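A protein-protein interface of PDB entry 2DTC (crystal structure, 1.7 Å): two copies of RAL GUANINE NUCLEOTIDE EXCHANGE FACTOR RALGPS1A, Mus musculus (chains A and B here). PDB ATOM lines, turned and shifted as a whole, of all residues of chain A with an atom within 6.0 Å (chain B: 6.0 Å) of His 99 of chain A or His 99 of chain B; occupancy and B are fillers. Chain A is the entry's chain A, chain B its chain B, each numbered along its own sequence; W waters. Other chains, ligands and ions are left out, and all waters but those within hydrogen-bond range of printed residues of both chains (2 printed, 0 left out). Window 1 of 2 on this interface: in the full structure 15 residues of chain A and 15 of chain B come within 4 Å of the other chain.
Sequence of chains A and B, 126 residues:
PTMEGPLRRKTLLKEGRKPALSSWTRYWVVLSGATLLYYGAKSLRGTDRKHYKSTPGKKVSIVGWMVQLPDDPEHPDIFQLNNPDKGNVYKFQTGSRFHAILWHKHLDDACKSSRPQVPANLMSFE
Glu 4 of chain A touches His 99 of chain B, and with the chains exchanged His 99 of chain A touches Glu 4 of chain B. Trp 28 of chain A touches Ser 96 of chain B, and with the chains exchanged Ser 96 of chain A touches Trp 28 of chain B. His 99 of chain A touches Gly 5 of chain B, but with the chains exchanged Gly 5 of chain A does not touch His 99 of chain B (4.1 Å). His 99 of chain A touches its own counterpart, His 99 of chain B. 17 positions are printed for both chains.
Of the 17 printed residues of chain B, 7 touch a printed residue of chain A. Of the 17 printed residues of chain A, 6 touch a printed residue of chain B. Hydrophobic or aromatic side chains of chain A that line the printed part of chain B: Met 3, Trp 28, Phe 98 and His 99. Along chain A the printed residues that touch a printed residue of chain B span positions 3 to 99.
Among the printed residues, pairs that only touch across the chains: Met 3 of chain A with Phe 98 of chain B, Glu 4 of chain A with Phe 98 of chain B, Trp 28 of chain A with Ser 96 of chain B, Ser 96 of chain A with Trp 28 of chain B, Phe 98 of chain A with Met 3 of chain B, Phe 98 of chain A with Glu 4 of chain B, His 99 of chain A with Gly 5 of chain B and His 99 of chain A with His 99 of chain B.
Water W2 lies within hydrogen-bond range of the backbone NH (N) of Phe 98 of chain A, the side-chain carboxylate (OE1) of Glu 4 of chain B and the backbone NH (N) of Arg 97 of chain A. Water W1 lies within hydrogen-bond range of N of Phe 98 of chain B (3.0 Å), OE1 of Glu 4 of chain A (3.2 Å) and N of Arg 97 of chain B (3.4 Å).
The side-chain carboxylate (OE1) of Glu 4 of chain A lies within hydrogen-bond range of the indole nitrogen (NE1) of Trp 28 of chain A (2.9 Å). The side-chain hydroxyl of Thr 94 of chain A is in hydrogen-bond range of the backbone carbonyl oxygen of Ser 96 of chain A, at 2.8 Å. The backbone NH (N) of His 99 of chain A sits at hydrogen-bond distance from the side-chain hydroxyl (OG) of Ser 96 of chain A, 2.9 Å away. OE1 of Glu 4 of chain B lies within hydrogen-bond range of NE1 of Trp 28 of chain B (2.9 Å). The side-chain hydroxyl (OG1) of Thr 94 of chain B lies within hydrogen-bond range of the backbone carbonyl oxygen (O) of Ser 96 of chain B (2.7 Å). The backbone NH (N) of His 99 of chain B sits at hydrogen-bond distance from the side-chain hydroxyl (OG) of Ser 96 of chain B, at 3.1 Å.
Of chain B, only Glu 4 (2.8 Å), Gly 5 (3.9 Å) and His 99 (3.7 Å) come within 4 Å of His 99 of chain A. His 99 of chain B touches two residues of chain A. Of the printed residues of chain A, Phe 98 of chain B touches Met 3 (3.6 Å) and Glu 4 (3.7 Å). Of the printed residues of chain B, Glu 4 of chain A touches Phe 98 (3.7 Å) and His 99 (2.8 Å). Gly 95 of chain B touches none of the printed residues of chain A. The nearest residue of chain B that does not touch His 99 of chain A is Trp 28 of chain B (4.4 Å). The nearest residue of chain A that does not touch His 99 of chain B is Gly 5 of chain A (4.1 Å). The nearest printed residue of chain B that does not touch Trp 28 of chain A is Gly 95 of chain B (4.5 Å).
The backbone carbonyl oxygen (O) of Glu 4 of chain A lies within hydrogen-bond range of a ring nitrogen (NE2) of His 99 of chain B (2.8 Å). A ring nitrogen (NE2) of His 99 of chain A sits at hydrogen-bond distance from the backbone carbonyl oxygen of Glu 4 of chain B (2.8 Å).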
ATOM      1  N   MET A   3      23.377  -2.503  21.746  1.00  0.00           N
ATOM      2  CA  MET A   3      24.338  -3.594  21.793  1.00  0.00           C
ATOM      3  C   MET A   3      25.377  -3.331  20.704  1.00  0.00           C
ATOM      4  O   MET A   3      25.043  -2.772  19.660  1.00  0.00           O
ATOM      5  CB  MET A   3      23.606  -4.930  21.524  1.00  0.00           C
ATOM      6  CG  MET A   3      24.475  -6.183  21.616  1.00  0.00           C
ATOM      7  SD  MET A   3      25.359  -6.349  23.339  1.00  0.00           S
ATOM      8  CE  MET A   3      26.633  -7.725  22.796  1.00  0.00           C
ATOM      9  N   GLU A   4      26.622  -3.709  20.979  1.00  0.00           N
ATOM     10  CA  GLU A   4      27.735  -3.542  20.028  1.00  0.00           C
ATOM     11  C   GLU A   4      28.703  -4.689  20.242  1.00  0.00           C
ATOM     12  O   GLU A   4      28.783  -5.260  21.338  1.00  0.00           O
ATOM     13  CB  GLU A   4      28.547  -2.269  20.293  1.00  0.00           C
ATOM     14  CG  GLU A   4      27.818  -0.971  20.170  1.00  0.00           C
ATOM     15  CD  GLU A   4      28.766   0.225  20.024  1.00  0.00           C
ATOM     16  OE1 GLU A   4      29.895   0.063  19.504  1.00  0.00           O
ATOM     17  OE2 GLU A   4      28.357   1.345  20.393  1.00  0.00           O
ATOM     18  N   GLY A   5      29.446  -5.026  19.199  1.00  0.00           N
ATOM     19  CA  GLY A   5      30.442  -6.061  19.364  1.00  0.00           C
ATOM     20  C   GLY A   5      30.983  -6.600  18.065  1.00  0.00           C
ATOM     21  O   GLY A   5      30.415  -6.366  16.999  1.00  0.00           O
ATOM     22  N   PRO A   6      32.078  -7.365  18.135  1.00  0.00           N
ATOM     23  CA  PRO A   6      32.684  -7.949  16.951  1.00  0.00           C
ATOM     24  C   PRO A   6      31.975  -9.238  16.589  1.00  0.00           C
ATOM     25  O   PRO A   6      31.942 -10.190  17.397  1.00  0.00           O
ATOM     26  CB  PRO A   6      34.118  -8.187  17.384  1.00  0.00           C
ATOM     27  CG  PRO A   6      33.980  -8.507  18.854  1.00  0.00           C
ATOM     28  CD  PRO A   6      32.909  -7.572  19.338  1.00  0.00           C
ATOM     29  N   TRP A  28      32.239  -5.028  12.854  1.00  0.00           N
ATOM     30  CA  TRP A  28      31.901  -4.509  14.172  1.00  0.00           C
ATOM     31  C   TRP A  28      30.424  -4.213  13.887  1.00  0.00           C
ATOM     32  O   TRP A  28      30.101  -3.546  12.892  1.00  0.00           O
ATOM     33  CB  TRP A  28      32.607  -3.203  14.541  1.00  0.00           C
ATOM     34  CG  TRP A  28      32.243  -2.792  15.962  1.00  0.00           C
ATOM     35  CD1 TRP A  28      31.280  -1.896  16.340  1.00  0.00           C
ATOM     36  CD2 TRP A  28      32.832  -3.283  17.171  1.00  0.00           C
ATOM     37  NE1 TRP A  28      31.242  -1.792  17.716  1.00  0.00           N
ATOM     38  CE2 TRP A  28      32.185  -2.633  18.246  1.00  0.00           C
ATOM     39  CE3 TRP A  28      33.841  -4.212  17.446  1.00  0.00           C
ATOM     40  CZ2 TRP A  28      32.520  -2.884  19.580  1.00  0.00           C
ATOM     41  CZ3 TRP A  28      34.183  -4.462  18.770  1.00  0.00           C
ATOM     42  CH2 TRP A  28      33.524  -3.802  19.818  1.00  0.00           C
ATOM     43  N   PHE A  79      24.144 -17.544  16.209  1.00  0.00           N
ATOM     44  CA  PHE A  79      22.735 -17.197  16.243  1.00  0.00           C
ATOM     45  C   PHE A  79      22.397 -16.986  14.775  1.00  0.00           C
ATOM     46  O   PHE A  79      23.281 -16.688  13.973  1.00  0.00           O
ATOM     47  CB  PHE A  79      22.390 -15.986  17.126  1.00  0.00           C
ATOM     48  CG  PHE A  79      22.941 -14.674  16.668  1.00  0.00           C
ATOM     49  CD1 PHE A  79      22.287 -13.907  15.689  1.00  0.00           C
ATOM     50  CD2 PHE A  79      24.051 -14.133  17.317  1.00  0.00           C
ATOM     51  CE1 PHE A  79      22.739 -12.617  15.384  1.00  0.00           C
ATOM     52  CE2 PHE A  79      24.497 -12.845  17.011  1.00  0.00           C
ATOM     53  CZ  PHE A  79      23.843 -12.092  16.051  1.00  0.00           C
ATOM     54  N   THR A  94      29.694 -15.207  17.451  1.00  0.00           N
ATOM     55  CA  THR A  94      29.946 -14.161  18.434  1.00  0.00           C
ATOM     56  C   THR A  94      31.186 -14.417  19.290  1.00  0.00           C
ATOM     57  O   THR A  94      31.600 -13.538  20.048  1.00  0.00           O
ATOM     58  CB  THR A  94      28.790 -14.021  19.446  1.00  0.00           C
ATOM     59  OG1 THR A  94      28.735 -15.212  20.249  1.00  0.00           O
ATOM     60  CG2 THR A  94      27.467 -13.794  18.755  1.00  0.00           C
ATOM     61  N   GLY A  95      31.765 -15.616  19.194  1.00  0.00           N
ATOM     62  CA  GLY A  95      32.929 -15.918  20.016  1.00  0.00           C
ATOM     63  C   GLY A  95      32.595 -16.658  21.317  1.00  0.00           C
ATOM     64  O   GLY A  95      33.483 -17.284  21.915  1.00  0.00           O
ATOM     65  N   SER A  96      31.346 -16.593  21.773  1.00  0.00           N
ATOM     66  CA  SER A  96      30.970 -17.318  23.005  1.00  0.00           C
ATOM     67  C   SER A  96      29.476 -17.584  23.112  1.00  0.00           C
ATOM     68  O   SER A  96      28.666 -16.839  22.569  1.00  0.00           O
ATOM     69  CB  SER A  96      31.410 -16.552  24.247  1.00  0.00           C
ATOM     70  OG  SER A  96      30.600 -15.403  24.441  1.00  0.00           O
ATOM     71  N   ARG A  97      29.111 -18.667  23.789  1.00  0.00           N
ATOM     72  CA  ARG A  97      27.699 -18.953  23.984  1.00  0.00           C
ATOM     73  C   ARG A  97      27.082 -17.758  24.717  1.00  0.00           C
ATOM     74  O   ARG A  97      25.990 -17.311  24.364  1.00  0.00           O
ATOM     75  CB  ARG A  97      27.520 -20.231  24.815  1.00  0.00           C
ATOM     76  CG  ARG A  97      26.087 -20.500  25.220  1.00  0.00           C
ATOM     77  CD  ARG A  97      25.193 -20.883  24.023  1.00  0.00           C
ATOM     78  NE  ARG A  97      23.814 -21.135  24.450  1.00  0.00           N
ATOM     79  CZ  ARG A  97      22.823 -21.515  23.644  1.00  0.00           C
ATOM     80  NH1 ARG A  97      23.035 -21.695  22.342  1.00  0.00           N
ATOM     81  NH2 ARG A  97      21.613 -21.733  24.149  1.00  0.00           N
ATOM     82  N   PHE A  98      27.772 -17.233  25.734  1.00  0.00           N
ATOM     83  CA  PHE A  98      27.226 -16.073  26.465  1.00  0.00           C
ATOM     84  C   PHE A  98      26.897 -14.898  25.544  1.00  0.00           C
ATOM     85  O   PHE A  98      25.816 -14.319  25.635  1.00  0.00           O
ATOM     86  CB  PHE A  98      28.184 -15.564  27.552  1.00  0.00           C
ATOM     87  CG  PHE A  98      27.600 -14.435  28.384  1.00  0.00           C
ATOM     88  CD1 PHE A  98      26.830 -14.711  29.507  1.00  0.00           C
ATOM     89  CD2 PHE A  98      27.768 -13.106  28.001  1.00  0.00           C
ATOM     90  CE1 PHE A  98      26.232 -13.680  30.229  1.00  0.00           C
ATOM     91  CE2 PHE A  98      27.183 -12.083  28.705  1.00  0.00           C
ATOM     92  CZ  PHE A  98      26.408 -12.369  29.827  1.00  0.00           C
ATOM     93  N   HIS A  99      27.803 -14.531  24.649  1.00  0.00           N
ATOM     94  CA  HIS A  99      27.476 -13.416  23.763  1.00  0.00           C
ATOM     95  C   HIS A  99      26.385 -13.768  22.739  1.00  0.00           C
ATOM     96  O   HIS A  99      25.611 -12.905  22.334  1.00  0.00           O
ATOM     97  CB  HIS A  99      28.750 -12.892  23.104  1.00  0.00           C
ATOM     98  CG  HIS A  99      29.594 -12.085  24.043  1.00  0.00           C
ATOM     99  ND1 HIS A  99      29.689 -10.713  23.965  1.00  0.00           N
ATOM    100  CD2 HIS A  99      30.273 -12.446  25.160  1.00  0.00           C
ATOM    101  CE1 HIS A  99      30.386 -10.263  24.994  1.00  0.00           C
ATOM    102  NE2 HIS A  99      30.750 -11.295  25.734  1.00  0.00           N
ATOM    103  N   ALA A 100      26.295 -15.032  22.339  1.00  0.00           N
ATOM    104  CA  ALA A 100      25.239 -15.417  21.414  1.00  0.00           C
ATOM    105  C   ALA A 100      23.891 -15.192  22.115  1.00  0.00           C
ATOM    106  O   ALA A 100      22.944 -14.690  21.512  1.00  0.00           O
ATOM    107  CB  ALA A 100      25.382 -16.907  20.991  1.00  0.00           C
ATOM    108  N   ILE A 101      23.808 -15.572  23.389  1.00  0.00           N
ATOM    109  CA  ILE A 101      22.572 -15.388  24.139  1.00  0.00           C
ATOM    110  C   ILE A 101      22.265 -13.907  24.309  1.00  0.00           C
ATOM    111  O   ILE A 101      21.123 -13.492  24.158  1.00  0.00           O
ATOM    112  CB  ILE A 101      22.650 -16.050  25.527  1.00  0.00           C
ATOM    113  CG1 ILE A 101      22.625 -17.573  25.352  1.00  0.00           C
ATOM    114  CG2 ILE A 101      21.457 -15.601  26.393  1.00  0.00           C
ATOM    115  CD1 ILE A 101      22.888 -18.342  26.635  1.00  0.00           C
ATOM    116  N   LEU A 102      23.292 -13.121  24.619  1.00  0.00           N
ATOM    117  CA  LEU A 102      23.134 -11.681  24.816  1.00  0.00           C
ATOM    118  C   LEU A 102      22.638 -11.012  23.527  1.00  0.00           C
ATOM    119  O   LEU A 102      21.680 -10.242  23.557  1.00  0.00           O
ATOM    120  CB  LEU A 102      24.472 -11.085  25.279  1.00  0.00           C
ATOM    121  CG  LEU A 102      24.544  -9.594  25.600  1.00  0.00           C
ATOM    122  CD1 LEU A 102      23.466  -9.206  26.605  1.00  0.00           C
ATOM    123  CD2 LEU A 102      25.921  -9.288  26.158  1.00  0.00           C
ATOM    124  N   TRP A 103      23.280 -11.312  22.395  1.00  0.00           N
ATOM    125  CA  TRP A 103      22.850 -10.729  21.129  1.00  0.00           C
ATOM    126  C   TRP A 103      21.432 -11.165  20.801  1.00  0.00           C
ATOM    127  O   TRP A 103      20.637 -10.363  20.321  1.00  0.00           O
ATOM    128  CB  TRP A 103      23.791 -11.130  19.974  1.00  0.00           C
ATOM    129  CG  TRP A 103      24.993 -10.256  19.837  1.00  0.00           C
ATOM    130  CD1 TRP A 103      26.274 -10.492  20.311  1.00  0.00           C
ATOM    131  CD2 TRP A 103      25.039  -9.002  19.154  1.00  0.00           C
ATOM    132  NE1 TRP A 103      27.113  -9.445  19.944  1.00  0.00           N
ATOM    133  CE2 TRP A 103      26.376  -8.524  19.231  1.00  0.00           C
ATOM    134  CE3 TRP A 103      24.076  -8.233  18.473  1.00  0.00           C
ATOM    135  CZ2 TRP A 103      26.769  -7.311  18.650  1.00  0.00           C
ATOM    136  CZ3 TRP A 103      24.468  -7.024  17.895  1.00  0.00           C
ATOM    137  CH2 TRP A 103      25.804  -6.577  17.985  1.00  0.00           C
ATOM    138  N   HIS A 104      21.114 -12.440  21.039  1.00  0.00           N
ATOM    139  CA  HIS A 104      19.773 -12.927  20.752  1.00  0.00           C
ATOM    140  C   HIS A 104      18.734 -12.125  21.528  1.00  0.00           C
ATOM    141  O   HIS A 104      17.699 -11.749  20.980  1.00  0.00           O
ATOM    142  CB  HIS A 104      19.643 -14.417  21.101  1.00  0.00           C
ATOM    143  CG  HIS A 104      18.233 -14.914  21.047  1.00  0.00           C
ATOM    144  ND1 HIS A 104      17.418 -14.963  22.157  1.00  0.00           N
ATOM    145  CD2 HIS A 104      17.466 -15.305  19.999  1.00  0.00           C
ATOM    146  CE1 HIS A 104      16.209 -15.360  21.798  1.00  0.00           C
ATOM    147  NE2 HIS A 104      16.211 -15.575  20.493  1.00  0.00           N
ATOM    148  N   MET B   3      27.875 -11.829  33.402  1.00  0.00           N
ATOM    149  CA  MET B   3      28.594 -11.204  32.311  1.00  0.00           C
ATOM    150  C   MET B   3      29.830 -12.046  32.034  1.00  0.00           C
ATOM    151  O   MET B   3      30.373 -12.664  32.956  1.00  0.00           O
ATOM    152  CB  MET B   3      28.983  -9.771  32.725  1.00  0.00           C
ATOM    153  CG  MET B   3      29.700  -8.958  31.661  1.00  0.00           C
ATOM    154  SD  MET B   3      28.625  -8.751  30.074  1.00  0.00           S
ATOM    155  CE  MET B   3      30.046  -8.028  28.953  1.00  0.00           C
ATOM    156  N   GLU B   4      30.245 -12.104  30.765  1.00  0.00           N
ATOM    157  CA  GLU B   4      31.439 -12.846  30.357  1.00  0.00           C
ATOM    158  C   GLU B   4      32.059 -12.112  29.194  1.00  0.00           C
ATOM    159  O   GLU B   4      31.366 -11.440  28.426  1.00  0.00           O
ATOM    160  CB  GLU B   4      31.123 -14.261  29.827  1.00  0.00           C
ATOM    161  CG  GLU B   4      30.478 -15.230  30.793  1.00  0.00           C
ATOM    162  CD  GLU B   4      30.581 -16.687  30.322  1.00  0.00           C
ATOM    163  OE1 GLU B   4      31.521 -17.043  29.567  1.00  0.00           O
ATOM    164  OE2 GLU B   4      29.733 -17.495  30.739  1.00  0.00           O
ATOM    165  N   GLY B   5      33.368 -12.243  29.049  1.00  0.00           N
ATOM    166  CA  GLY B   5      33.973 -11.622  27.897  1.00  0.00           C
ATOM    167  C   GLY B   5      35.465 -11.580  27.993  1.00  0.00           C
ATOM    168  O   GLY B   5      36.025 -11.842  29.060  1.00  0.00           O
ATOM    169  N   PRO B   6      36.132 -11.227  26.885  1.00  0.00           N
ATOM    170  CA  PRO B   6      37.578 -11.142  26.863  1.00  0.00           C
ATOM    171  C   PRO B   6      38.008  -9.795  27.423  1.00  0.00           C
ATOM    172  O   PRO B   6      37.556  -8.750  26.957  1.00  0.00           O
ATOM    173  CB  PRO B   6      37.910 -11.296  25.391  1.00  0.00           C
ATOM    174  CG  PRO B   6      36.738 -10.652  24.706  1.00  0.00           C
ATOM    175  CD  PRO B   6      35.560 -11.082  25.527  1.00  0.00           C
ATOM    176  N   TRP B  28      39.845 -14.466  29.885  1.00  0.00           N
ATOM    177  CA  TRP B  28      38.425 -14.574  29.596  1.00  0.00           C
ATOM    178  C   TRP B  28      37.953 -14.427  31.035  1.00  0.00           C
ATOM    179  O   TRP B  28      38.446 -15.144  31.930  1.00  0.00           O
ATOM    180  CB  TRP B  28      37.990 -15.939  29.072  1.00  0.00           C
ATOM    181  CG  TRP B  28      36.506 -15.935  28.782  1.00  0.00           C
ATOM    182  CD1 TRP B  28      35.510 -16.362  29.608  1.00  0.00           C
ATOM    183  CD2 TRP B  28      35.861 -15.441  27.596  1.00  0.00           C
ATOM    184  NE1 TRP B  28      34.280 -16.173  29.007  1.00  0.00           N
ATOM    185  CE2 TRP B  28      34.467 -15.608  27.774  1.00  0.00           C
ATOM    186  CE3 TRP B  28      36.329 -14.879  26.407  1.00  0.00           C
ATOM    187  CZ2 TRP B  28      33.530 -15.233  26.802  1.00  0.00           C
ATOM    188  CZ3 TRP B  28      35.398 -14.503  25.426  1.00  0.00           C
ATOM    189  CH2 TRP B  28      34.016 -14.682  25.635  1.00  0.00           C
ATOM    190  N   PHE B  79      38.020   0.460  32.356  1.00  0.00           N
ATOM    191  CA  PHE B  79      37.325   0.664  33.624  1.00  0.00           C
ATOM    192  C   PHE B  79      38.324   0.286  34.701  1.00  0.00           C
ATOM    193  O   PHE B  79      39.288  -0.440  34.444  1.00  0.00           O
ATOM    194  CB  PHE B  79      35.988  -0.087  33.763  1.00  0.00           C
ATOM    195  CG  PHE B  79      36.085  -1.585  33.793  1.00  0.00           C
ATOM    196  CD1 PHE B  79      36.386  -2.269  34.973  1.00  0.00           C
ATOM    197  CD2 PHE B  79      35.792  -2.320  32.648  1.00  0.00           C
ATOM    198  CE1 PHE B  79      36.381  -3.687  34.986  1.00  0.00           C
ATOM    199  CE2 PHE B  79      35.785  -3.711  32.667  1.00  0.00           C
ATOM    200  CZ  PHE B  79      36.077  -4.391  33.824  1.00  0.00           C
ATOM    201  N   THR B  94      38.512  -3.453  27.562  1.00  0.00           N
ATOM    202  CA  THR B  94      37.445  -4.312  27.040  1.00  0.00           C
ATOM    203  C   THR B  94      37.359  -4.352  25.515  1.00  0.00           C
ATOM    204  O   THR B  94      36.586  -5.142  24.965  1.00  0.00           O
ATOM    205  CB  THR B  94      36.043  -3.820  27.456  1.00  0.00           C
ATOM    206  OG1 THR B  94      35.776  -2.578  26.773  1.00  0.00           O
ATOM    207  CG2 THR B  94      35.926  -3.627  28.962  1.00  0.00           C
ATOM    208  N   GLY B  95      38.103  -3.481  24.844  1.00  0.00           N
ATOM    209  CA  GLY B  95      38.031  -3.416  23.389  1.00  0.00           C
ATOM    210  C   GLY B  95      37.077  -2.336  22.871  1.00  0.00           C
ATOM    211  O   GLY B  95      37.184  -1.915  21.713  1.00  0.00           O
ATOM    212  N   SER B  96      36.125  -1.895  23.692  1.00  0.00           N
ATOM    213  CA  SER B  96      35.201  -0.838  23.244  1.00  0.00           C
ATOM    214  C   SER B  96      34.554  -0.073  24.396  1.00  0.00           C
ATOM    215  O   SER B  96      34.384  -0.589  25.509  1.00  0.00           O
ATOM    216  CB  SER B  96      34.086  -1.420  22.378  1.00  0.00           C
ATOM    217  OG  SER B  96      33.235  -2.260  23.151  1.00  0.00           O
ATOM    218  N   ARG B  97      34.208   1.175  24.139  1.00  0.00           N
ATOM    219  CA  ARG B  97      33.563   1.947  25.176  1.00  0.00           C
ATOM    220  C   ARG B  97      32.263   1.252  25.593  1.00  0.00           C
ATOM    221  O   ARG B  97      31.946   1.192  26.779  1.00  0.00           O
ATOM    222  CB  ARG B  97      33.282   3.358  24.658  1.00  0.00           C
ATOM    223  CG  ARG B  97      32.407   4.157  25.552  1.00  0.00           C
ATOM    224  CD  ARG B  97      33.122   4.582  26.822  1.00  0.00           C
ATOM    225  NE  ARG B  97      32.280   5.496  27.594  1.00  0.00           N
ATOM    226  CZ  ARG B  97      32.648   6.061  28.740  1.00  0.00           C
ATOM    227  NH1 ARG B  97      33.846   5.801  29.258  1.00  0.00           N
ATOM    228  NH2 ARG B  97      31.824   6.896  29.363  1.00  0.00           N
ATOM    229  N   PHE B  98      31.508   0.737  24.627  1.00  0.00           N
ATOM    230  CA  PHE B  98      30.253   0.062  24.963  1.00  0.00           C
ATOM    231  C   PHE B  98      30.495  -1.071  25.947  1.00  0.00           C
ATOM    232  O   PHE B  98      29.812  -1.175  26.958  1.00  0.00           O
ATOM    233  CB  PHE B  98      29.580  -0.532  23.725  1.00  0.00           C
ATOM    234  CG  PHE B  98      28.306  -1.265  24.046  1.00  0.00           C
ATOM    235  CD1 PHE B  98      27.119  -0.568  24.211  1.00  0.00           C
ATOM    236  CD2 PHE B  98      28.313  -2.645  24.262  1.00  0.00           C
ATOM    237  CE1 PHE B  98      25.945  -1.236  24.590  1.00  0.00           C
ATOM    238  CE2 PHE B  98      27.147  -3.320  24.644  1.00  0.00           C
ATOM    239  CZ  PHE B  98      25.969  -2.622  24.808  1.00  0.00           C
ATOM    240  N   HIS B  99      31.470  -1.928  25.665  1.00  0.00           N
ATOM    241  CA  HIS B  99      31.705  -3.009  26.609  1.00  0.00           C
ATOM    242  C   HIS B  99      32.232  -2.515  27.960  1.00  0.00           C
ATOM    243  O   HIS B  99      31.939  -3.131  28.999  1.00  0.00           O
ATOM    244  CB  HIS B  99      32.591  -4.078  25.962  1.00  0.00           C
ATOM    245  CG  HIS B  99      31.835  -4.944  25.008  1.00  0.00           C
ATOM    246  ND1 HIS B  99      31.358  -6.189  25.362  1.00  0.00           N
ATOM    247  CD2 HIS B  99      31.338  -4.686  23.772  1.00  0.00           C
ATOM    248  CE1 HIS B  99      30.595  -6.659  24.390  1.00  0.00           C
ATOM    249  NE2 HIS B  99      30.565  -5.766  23.414  1.00  0.00           N
ATOM    250  N   ALA B 100      32.969  -1.401  27.974  1.00  0.00           N
ATOM    251  CA  ALA B 100      33.427  -0.870  29.256  1.00  0.00           C
ATOM    252  C   ALA B 100      32.190  -0.451  30.056  1.00  0.00           C
ATOM    253  O   ALA B 100      32.117  -0.709  31.246  1.00  0.00           O
ATOM    254  CB  ALA B 100      34.359   0.334  29.064  1.00  0.00           C
ATOM    255  N   ILE B 101      31.227   0.202  29.395  1.00  0.00           N
ATOM    256  CA  ILE B 101      30.016   0.637  30.087  1.00  0.00           C
ATOM    257  C   ILE B 101      29.207  -0.552  30.589  1.00  0.00           C
ATOM    258  O   ILE B 101      28.713  -0.530  31.716  1.00  0.00           O
ATOM    259  CB  ILE B 101      29.138   1.533  29.168  1.00  0.00           C
ATOM    260  CG1 ILE B 101      29.854   2.874  28.952  1.00  0.00           C
ATOM    261  CG2 ILE B 101      27.772   1.786  29.804  1.00  0.00           C
ATOM    262  CD1 ILE B 101      29.322   3.653  27.773  1.00  0.00           C
ATOM    263  N   LEU B 102      29.096  -1.589  29.761  1.00  0.00           N
ATOM    264  CA  LEU B 102      28.347  -2.790  30.110  1.00  0.00           C
ATOM    265  C   LEU B 102      28.998  -3.492  31.306  1.00  0.00           C
ATOM    266  O   LEU B 102      28.317  -3.832  32.274  1.00  0.00           O
ATOM    267  CB  LEU B 102      28.252  -3.733  28.903  1.00  0.00           C
ATOM    268  CG  LEU B 102      27.429  -5.015  29.101  1.00  0.00           C
ATOM    269  CD1 LEU B 102      26.016  -4.676  29.548  1.00  0.00           C
ATOM    270  CD2 LEU B 102      27.392  -5.789  27.790  1.00  0.00           C
ATOM    271  N   TRP B 103      30.314  -3.696  31.252  1.00  0.00           N
ATOM    272  CA  TRP B 103      30.990  -4.338  32.375  1.00  0.00           C
ATOM    273  C   TRP B 103      30.842  -3.481  33.622  1.00  0.00           C
ATOM    274  O   TRP B 103      30.603  -4.000  34.707  1.00  0.00           O
ATOM    275  CB  TRP B 103      32.496  -4.552  32.090  1.00  0.00           C
ATOM    276  CG  TRP B 103      32.803  -5.834  31.354  1.00  0.00           C
ATOM    277  CD1 TRP B 103      32.991  -5.995  30.006  1.00  0.00           C
ATOM    278  CD2 TRP B 103      32.960  -7.136  31.940  1.00  0.00           C
ATOM    279  NE1 TRP B 103      33.270  -7.322  29.716  1.00  0.00           N
ATOM    280  CE2 TRP B 103      33.253  -8.040  30.890  1.00  0.00           C
ATOM    281  CE3 TRP B 103      32.877  -7.625  33.255  1.00  0.00           C
ATOM    282  CZ2 TRP B 103      33.469  -9.406  31.113  1.00  0.00           C
ATOM    283  CZ3 TRP B 103      33.087  -8.983  33.476  1.00  0.00           C
ATOM    284  CH2 TRP B 103      33.381  -9.858  32.413  1.00  0.00           C
ATOM    285  N   HIS B 104      30.972  -2.163  33.482  1.00  0.00           N
ATOM    286  CA  HIS B 104      30.865  -1.325  34.658  1.00  0.00           C
ATOM    287  C   HIS B 104      29.521  -1.520  35.340  1.00  0.00           C
ATOM    288  O   HIS B 104      29.455  -1.630  36.564  1.00  0.00           O
ATOM    289  CB  HIS B 104      31.060   0.139  34.302  1.00  0.00           C
ATOM    290  CG  HIS B 104      30.708   1.073  35.414  1.00  0.00           C
ATOM    291  ND1 HIS B 104      29.458   1.634  35.545  1.00  0.00           N
ATOM    292  CD2 HIS B 104      31.424   1.497  36.484  1.00  0.00           C
ATOM    293  CE1 HIS B 104      29.415   2.365  36.647  1.00  0.00           C
ATOM    294  NE2 HIS B 104      30.598   2.299  37.236  1.00  0.00           N
HETATM  295  O   HOH W   1      31.825   1.240  21.705  1.00  0.00           O
HETATM  296  O   HOH W   2      30.169 -18.306  27.011  1.00  0.00           O
